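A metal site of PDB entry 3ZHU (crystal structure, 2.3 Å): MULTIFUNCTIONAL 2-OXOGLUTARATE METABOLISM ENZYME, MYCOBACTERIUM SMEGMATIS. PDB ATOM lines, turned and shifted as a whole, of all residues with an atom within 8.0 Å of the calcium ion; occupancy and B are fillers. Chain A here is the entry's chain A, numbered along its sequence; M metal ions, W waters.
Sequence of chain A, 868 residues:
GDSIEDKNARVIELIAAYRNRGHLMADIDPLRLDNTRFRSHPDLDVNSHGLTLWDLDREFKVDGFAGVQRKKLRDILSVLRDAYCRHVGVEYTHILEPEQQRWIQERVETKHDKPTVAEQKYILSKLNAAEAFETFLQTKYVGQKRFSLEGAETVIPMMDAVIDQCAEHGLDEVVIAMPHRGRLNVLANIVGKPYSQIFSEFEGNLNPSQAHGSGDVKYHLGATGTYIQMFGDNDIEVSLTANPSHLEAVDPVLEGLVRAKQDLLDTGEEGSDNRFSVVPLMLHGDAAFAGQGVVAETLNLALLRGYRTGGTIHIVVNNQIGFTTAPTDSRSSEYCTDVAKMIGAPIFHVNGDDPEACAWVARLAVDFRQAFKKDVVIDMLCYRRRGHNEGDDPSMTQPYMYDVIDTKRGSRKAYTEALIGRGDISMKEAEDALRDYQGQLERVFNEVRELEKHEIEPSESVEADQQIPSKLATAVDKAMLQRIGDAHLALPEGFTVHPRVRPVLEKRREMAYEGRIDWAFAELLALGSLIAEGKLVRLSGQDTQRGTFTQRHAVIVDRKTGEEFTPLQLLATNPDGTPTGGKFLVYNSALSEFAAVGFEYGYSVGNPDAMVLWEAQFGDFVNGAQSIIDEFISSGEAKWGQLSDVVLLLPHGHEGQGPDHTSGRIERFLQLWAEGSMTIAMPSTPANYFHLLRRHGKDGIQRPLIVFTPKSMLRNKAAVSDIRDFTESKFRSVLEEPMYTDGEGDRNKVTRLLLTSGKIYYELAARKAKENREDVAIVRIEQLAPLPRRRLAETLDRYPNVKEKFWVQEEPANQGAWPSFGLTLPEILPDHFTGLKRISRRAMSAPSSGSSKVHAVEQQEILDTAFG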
ATOM      1  N   GLN A 466      33.929 -11.066  21.621  1.00  0.00           N
ATOM      2  CA  GLN A 466      32.494 -11.253  21.408  1.00  0.00           C
ATOM      3  C   GLN A 466      32.207 -12.752  21.197  1.00  0.00           C
ATOM      4  O   GLN A 466      32.557 -13.314  20.151  1.00  0.00           O
ATOM      5  CB  GLN A 466      31.988 -10.404  20.229  1.00  0.00           C
ATOM      6  CG  GLN A 466      32.141  -8.896  20.431  1.00  0.00           C
ATOM      7  CD  GLN A 466      31.352  -8.113  19.419  1.00  0.00           C
ATOM      8  OE1 GLN A 466      30.128  -8.013  19.499  1.00  0.00           O
ATOM      9  NE2 GLN A 466      32.036  -7.509  18.447  1.00  0.00           N
ATOM     10  N   LYS A 535      12.127  -5.281  16.981  1.00  0.00           N
ATOM     11  CA  LYS A 535      13.383  -4.784  16.405  1.00  0.00           C
ATOM     12  C   LYS A 535      13.195  -3.726  15.314  1.00  0.00           C
ATOM     13  O   LYS A 535      12.317  -3.853  14.454  1.00  0.00           O
ATOM     14  CB  LYS A 535      14.199  -5.942  15.824  1.00  0.00           C
ATOM     15  CG  LYS A 535      15.684  -5.718  15.958  1.00  0.00           C
ATOM     16  CD  LYS A 535      16.507  -6.829  15.337  1.00  0.00           C
ATOM     17  CE  LYS A 535      17.981  -6.553  15.520  1.00  0.00           C
ATOM     18  NZ  LYS A 535      18.376  -6.540  16.961  1.00  0.00           N
ATOM     19  N   PRO A 608      23.155  -0.050  17.809  1.00  0.00           N
ATOM     20  CA  PRO A 608      23.566  -1.470  17.822  1.00  0.00           C
ATOM     21  C   PRO A 608      22.385  -2.438  17.917  1.00  0.00           C
ATOM     22  O   PRO A 608      22.564  -3.619  17.580  1.00  0.00           O
ATOM     23  CB  PRO A 608      24.462  -1.571  19.065  1.00  0.00           C
ATOM     24  CG  PRO A 608      24.791  -0.149  19.448  1.00  0.00           C
ATOM     25  CD  PRO A 608      23.626   0.660  19.019  1.00  0.00           C
ATOM     26  N   ALA A 610      19.606  -2.095  16.149  1.00  0.00           N
ATOM     27  CA  ALA A 610      18.940  -2.121  14.865  1.00  0.00           C
ATOM     28  C   ALA A 610      19.480  -3.251  13.975  1.00  0.00           C
ATOM     29  O   ALA A 610      20.633  -3.666  14.117  1.00  0.00           O
ATOM     30  CB  ALA A 610      19.117  -0.777  14.171  1.00  0.00           C
ATOM     31  N   MET A 611      18.622  -3.739  13.078  1.00  0.00           N
ATOM     32  CA  MET A 611      18.916  -4.696  12.025  1.00  0.00           C
ATOM     33  C   MET A 611      19.128  -3.817  10.776  1.00  0.00           C
ATOM     34  O   MET A 611      18.181  -3.187  10.293  1.00  0.00           O
ATOM     35  CB  MET A 611      17.760  -5.721  11.871  1.00  0.00           C
ATOM     36  CG  MET A 611      18.012  -6.789  10.832  1.00  0.00           C
ATOM     37  SD  MET A 611      19.080  -8.140  11.354  1.00  0.00           S
ATOM     38  CE  MET A 611      19.119  -9.093   9.891  1.00  0.00           C
ATOM     39  N   SER A 644      30.079  -2.833  14.674  1.00  0.00           N
ATOM     40  CA  SER A 644      29.067  -2.676  13.655  1.00  0.00           C
ATOM     41  C   SER A 644      28.453  -4.017  13.323  1.00  0.00           C
ATOM     42  O   SER A 644      29.174  -4.991  13.173  1.00  0.00           O
ATOM     43  CB  SER A 644      29.651  -2.052  12.402  1.00  0.00           C
ATOM     44  OG  SER A 644      28.685  -1.859  11.378  1.00  0.00           O
ATOM     45  N   ASP A 645      27.130  -4.067  13.173  1.00  0.00           N
ATOM     46  CA  ASP A 645      26.394  -5.290  12.825  1.00  0.00           C
ATOM     47  C   ASP A 645      25.799  -5.166  11.410  1.00  0.00           C
ATOM     48  O   ASP A 645      24.832  -5.877  11.083  1.00  0.00           O
ATOM     49  CB  ASP A 645      25.279  -5.495  13.874  1.00  0.00           C
ATOM     50  CG  ASP A 645      24.991  -6.945  14.220  1.00  0.00           C
ATOM     51  OD1 ASP A 645      25.944  -7.737  14.265  1.00  0.00           O
ATOM     52  OD2 ASP A 645      23.822  -7.261  14.514  1.00  0.00           O
ATOM     53  N   VAL A 646      26.365  -4.290  10.559  1.00  0.00           N
ATOM     54  CA  VAL A 646      25.867  -4.049   9.189  1.00  0.00           C
ATOM     55  C   VAL A 646      25.846  -5.346   8.350  1.00  0.00           C
ATOM     56  O   VAL A 646      26.774  -6.160   8.414  1.00  0.00           O
ATOM     57  CB  VAL A 646      26.615  -2.886   8.479  1.00  0.00           C
ATOM     58  CG1 VAL A 646      28.070  -3.256   8.107  1.00  0.00           C
ATOM     59  CG2 VAL A 646      25.833  -2.368   7.277  1.00  0.00           C
ATOM     60  N   VAL A 647      24.756  -5.551   7.619  1.00  0.00           N
ATOM     61  CA  VAL A 647      24.611  -6.695   6.726  1.00  0.00           C
ATOM     62  C   VAL A 647      24.818  -6.191   5.293  1.00  0.00           C
ATOM     63  O   VAL A 647      24.166  -5.234   4.894  1.00  0.00           O
ATOM     64  CB  VAL A 647      23.245  -7.441   6.861  1.00  0.00           C
ATOM     65  CG1 VAL A 647      23.210  -8.690   5.968  1.00  0.00           C
ATOM     66  CG2 VAL A 647      22.926  -7.789   8.308  1.00  0.00           C
ATOM     67  N   THR A 679      31.071 -12.380   9.582  1.00  0.00           N
ATOM     68  CA  THR A 679      30.460 -13.639   9.197  1.00  0.00           C
ATOM     69  C   THR A 679      30.279 -13.534   7.692  1.00  0.00           C
ATOM     70  O   THR A 679      29.869 -12.479   7.205  1.00  0.00           O
ATOM     71  CB  THR A 679      29.161 -13.926   9.994  1.00  0.00           C
ATOM     72  OG1 THR A 679      29.453 -13.896  11.386  1.00  0.00           O
ATOM     73  CG2 THR A 679      28.566 -15.292   9.658  1.00  0.00           C
ATOM     74  N   LEU A 692      19.863 -17.459   9.202  1.00  0.00           N
ATOM     75  CA  LEU A 692      21.101 -16.666   9.185  1.00  0.00           C
ATOM     76  C   LEU A 692      20.808 -15.196   9.594  1.00  0.00           C
ATOM     77  O   LEU A 692      21.536 -14.617  10.404  1.00  0.00           O
ATOM     78  CB  LEU A 692      21.756 -16.698   7.776  1.00  0.00           C
ATOM     79  CG  LEU A 692      23.036 -15.843   7.573  1.00  0.00           C
ATOM     80  CD1 LEU A 692      24.283 -16.569   8.109  1.00  0.00           C
ATOM     81  CD2 LEU A 692      23.213 -15.428   6.110  1.00  0.00           C
ATOM     82  N   LEU A 693      19.717 -14.607   9.039  1.00  0.00           N
ATOM     83  CA  LEU A 693      19.319 -13.228   9.344  1.00  0.00           C
ATOM     84  C   LEU A 693      18.831 -13.088  10.777  1.00  0.00           C
ATOM     85  O   LEU A 693      19.200 -12.126  11.451  1.00  0.00           O
ATOM     86  CB  LEU A 693      18.250 -12.724   8.372  1.00  0.00           C
ATOM     87  CG  LEU A 693      18.682 -12.458   6.917  1.00  0.00           C
ATOM     88  CD1 LEU A 693      17.488 -12.000   6.095  1.00  0.00           C
ATOM     89  CD2 LEU A 693      19.779 -11.400   6.840  1.00  0.00           C
ATOM     90  N   ARG A 694      17.999 -14.052  11.249  1.00  0.00           N
ATOM     91  CA  ARG A 694      17.464 -14.056  12.609  1.00  0.00           C
ATOM     92  C   ARG A 694      18.579 -14.247  13.627  1.00  0.00           C
ATOM     93  O   ARG A 694      18.595 -13.537  14.636  1.00  0.00           O
ATOM     94  CB  ARG A 694      16.366 -15.085  12.768  1.00  0.00           C
ATOM     95  CG  ARG A 694      15.045 -14.508  12.253  1.00  0.00           C
ATOM     96  CD  ARG A 694      13.821 -15.336  12.556  1.00  0.00           C
ATOM     97  NE  ARG A 694      13.615 -15.631  13.979  1.00  0.00           N
ATOM     98  CZ  ARG A 694      13.072 -14.802  14.874  1.00  0.00           C
ATOM     99  NH1 ARG A 694      12.732 -13.571  14.522  1.00  0.00           N
ATOM    100  NH2 ARG A 694      12.898 -15.191  16.121  1.00  0.00           N
ATOM    101  N   ARG A 695      19.552 -15.164  13.349  1.00  0.00           N
ATOM    102  CA  ARG A 695      20.698 -15.386  14.237  1.00  0.00           C
ATOM    103  C   ARG A 695      21.494 -14.078  14.343  1.00  0.00           C
ATOM    104  O   ARG A 695      21.790 -13.644  15.458  1.00  0.00           O
ATOM    105  CB  ARG A 695      21.581 -16.558  13.740  1.00  0.00           C
ATOM    106  CG  ARG A 695      22.787 -16.867  14.646  1.00  0.00           C
ATOM    107  CD  ARG A 695      23.631 -18.023  14.107  1.00  0.00           C
ATOM    108  NE  ARG A 695      24.341 -17.679  12.863  1.00  0.00           N
ATOM    109  CZ  ARG A 695      25.436 -18.311  12.421  1.00  0.00           C
ATOM    110  NH1 ARG A 695      25.973 -19.301  13.118  1.00  0.00           N
ATOM    111  NH2 ARG A 695      26.003 -17.930  11.287  1.00  0.00           N
ATOM    112  N   HIS A 696      21.751 -13.415  13.192  1.00  0.00           N
ATOM    113  CA  HIS A 696      22.484 -12.156  13.144  1.00  0.00           C
ATOM    114  C   HIS A 696      21.818 -11.047  13.955  1.00  0.00           C
ATOM    115  O   HIS A 696      22.508 -10.323  14.667  1.00  0.00           O
ATOM    116  CB  HIS A 696      22.660 -11.689  11.693  1.00  0.00           C
ATOM    117  CG  HIS A 696      23.473 -10.438  11.586  1.00  0.00           C
ATOM    118  ND1 HIS A 696      24.852 -10.465  11.750  1.00  0.00           N
ATOM    119  CD2 HIS A 696      23.082  -9.163  11.409  1.00  0.00           C
ATOM    120  CE1 HIS A 696      25.247  -9.210  11.623  1.00  0.00           C
ATOM    121  NE2 HIS A 696      24.218  -8.389  11.404  1.00  0.00           N
ATOM    122  N   GLY A 697      20.504 -10.918  13.860  1.00  0.00           N
ATOM    123  CA  GLY A 697      19.774  -9.899  14.586  1.00  0.00           C
ATOM    124  C   GLY A 697      19.538 -10.192  16.057  1.00  0.00           C
ATOM    125  O   GLY A 697      19.353  -9.249  16.828  1.00  0.00           O
ATOM    126  N   LYS A 698      19.571 -11.473  16.461  1.00  0.00           N
ATOM    127  CA  LYS A 698      19.270 -11.873  17.847  1.00  0.00           C
ATOM    128  C   LYS A 698      20.482 -12.357  18.690  1.00  0.00           C
ATOM    129  O   LYS A 698      20.326 -12.526  19.887  1.00  0.00           O
ATOM    130  CB  LYS A 698      18.217 -12.999  17.855  1.00  0.00           C
ATOM    131  CG  LYS A 698      16.866 -12.586  17.304  1.00  0.00           C
ATOM    132  CD  LYS A 698      15.926 -13.797  17.128  1.00  0.00           C
ATOM    133  CE  LYS A 698      15.320 -14.280  18.419  1.00  0.00           C
ATOM    134  NZ  LYS A 698      14.386 -13.289  19.002  1.00  0.00           N
ATOM    135  N   ASP A 699      21.661 -12.594  18.071  1.00  0.00           N
ATOM    136  CA  ASP A 699      22.819 -13.163  18.784  1.00  0.00           C
ATOM    137  C   ASP A 699      23.504 -12.240  19.826  1.00  0.00           C
ATOM    138  O   ASP A 699      24.349 -12.719  20.581  1.00  0.00           O
ATOM    139  CB  ASP A 699      23.884 -13.673  17.783  1.00  0.00           C
ATOM    140  CG  ASP A 699      24.448 -12.673  16.773  1.00  0.00           C
ATOM    141  OD1 ASP A 699      24.245 -11.441  16.958  1.00  0.00           O
ATOM    142  OD2 ASP A 699      25.121 -13.113  15.814  1.00  0.00           O
ATOM    143  N   GLY A 700      23.194 -10.942  19.823  1.00  0.00           N
ATOM    144  CA  GLY A 700      23.809  -9.981  20.736  1.00  0.00           C
ATOM    145  C   GLY A 700      25.215  -9.538  20.375  1.00  0.00           C
ATOM    146  O   GLY A 700      25.759  -8.671  21.038  1.00  0.00           O
ATOM    147  N   ILE A 701      25.810 -10.137  19.317  1.00  0.00           N
ATOM    148  CA  ILE A 701      27.143  -9.852  18.759  1.00  0.00           C
ATOM    149  C   ILE A 701      27.002  -8.731  17.744  1.00  0.00           C
ATOM    150  O   ILE A 701      26.015  -8.702  17.007  1.00  0.00           O
ATOM    151  CB  ILE A 701      27.746 -11.155  18.135  1.00  0.00           C
ATOM    152  CG1 ILE A 701      28.130 -12.176  19.239  1.00  0.00           C
ATOM    153  CG2 ILE A 701      28.961 -10.904  17.205  1.00  0.00           C
ATOM    154  CD1 ILE A 701      27.329 -13.384  19.142  1.00  0.00           C
ATOM    155  N   GLN A 702      27.964  -7.793  17.714  1.00  0.00           N
ATOM    156  CA  GLN A 702      27.955  -6.675  16.773  1.00  0.00           C
ATOM    157  C   GLN A 702      29.110  -6.853  15.836  1.00  0.00           C
ATOM    158  O   GLN A 702      30.217  -6.329  16.068  1.00  0.00           O
ATOM    159  CB  GLN A 702      28.028  -5.317  17.526  1.00  0.00           C
ATOM    160  CG  GLN A 702      27.028  -5.141  18.678  1.00  0.00           C
ATOM    161  CD  GLN A 702      25.604  -5.187  18.197  1.00  0.00           C
ATOM    162  OE1 GLN A 702      25.231  -4.569  17.188  1.00  0.00           O
ATOM    163  NE2 GLN A 702      24.772  -5.922  18.933  1.00  0.00           N
ATOM    164  N   ARG A 703      28.890  -7.680  14.805  1.00  0.00           N
ATOM    165  CA  ARG A 703      29.892  -7.986  13.795  1.00  0.00           C
ATOM    166  C   ARG A 703      29.239  -8.048  12.437  1.00  0.00           C
ATOM    167  O   ARG A 703      28.145  -8.604  12.331  1.00  0.00           O
ATOM    168  CB  ARG A 703      30.669  -9.263  14.114  1.00  0.00           C
ATOM    169  CG  ARG A 703      31.784  -8.995  15.116  1.00  0.00           C
ATOM    170  CD  ARG A 703      32.474 -10.225  15.596  1.00  0.00           C
ATOM    171  NE  ARG A 703      33.508  -9.867  16.567  1.00  0.00           N
ATOM    172  CZ  ARG A 703      34.215 -10.724  17.280  1.00  0.00           C
ATOM    173  NH1 ARG A 703      34.039 -12.033  17.121  1.00  0.00           N
ATOM    174  NH2 ARG A 703      35.111 -10.286  18.145  1.00  0.00           N
ATOM    175  N   PRO A 704      29.843  -7.423  11.396  1.00  0.00           N
ATOM    176  CA  PRO A 704      29.184  -7.392  10.080  1.00  0.00           C
ATOM    177  C   PRO A 704      28.938  -8.779   9.496  1.00  0.00           C
ATOM    178  O   PRO A 704      29.663  -9.738   9.816  1.00  0.00           O
ATOM    179  CB  PRO A 704      30.170  -6.595   9.220  1.00  0.00           C
ATOM    180  CG  PRO A 704      30.964  -5.816  10.170  1.00  0.00           C
ATOM    181  CD  PRO A 704      31.118  -6.692  11.364  1.00  0.00           C
ATOM    182  N   LEU A 705      27.890  -8.889   8.678  1.00  0.00           N
ATOM    183  CA  LEU A 705      27.500 -10.115   7.996  1.00  0.00           C
ATOM    184  C   LEU A 705      27.522  -9.845   6.484  1.00  0.00           C
ATOM    185  O   LEU A 705      26.854  -8.943   5.993  1.00  0.00           O
ATOM    186  CB  LEU A 705      26.113 -10.614   8.480  1.00  0.00           C
ATOM    187  CG  LEU A 705      25.411 -11.741   7.673  1.00  0.00           C
ATOM    188  CD1 LEU A 705      26.218 -13.063   7.653  1.00  0.00           C
ATOM    189  CD2 LEU A 705      24.002 -11.971   8.163  1.00  0.00           C
HETATM  190 CA    CA M   1      24.456  -9.439  15.517  1.00  0.00          CA
HETATM  191  O   HOH W   1      23.077  -8.354  17.219  1.00  0.00           O
HETATM  192  O   HOH W   2      25.938 -10.947  14.611  1.00  0.00           O
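N of Arg 703 lies close to OD1 of Asp 645, 3.0 Å away.
Water W2 lies within hydrogen-bond range of the side-chain carboxylate (OD2) of Asp 699 (2.6 Å) and a ring nitrogen (ND1) of His 696 (3.1 Å).
O of Ile 701 binds the calcium ion (2.3 Å).
Water W2 binds the calcium ion (2.3 Å).
O of His 696 binds the calcium ion (2.3 Å).
The calcium ion is bound by water W1 (2.4 Å).
OD1 of Asp 699 is bound to the calcium ion, at 2.5 Å.
OD2 of Asp 645 binds the calcium ion (2.5 Å).
The side-chain carboxylate (OD1) of Asp 645 binds the calcium ion.
Of the 24 residues printed, 4 come within 4 Å of the calcium ion.
Along chain A the residues within 4 Å of the calcium ion span positions 645 to 701.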
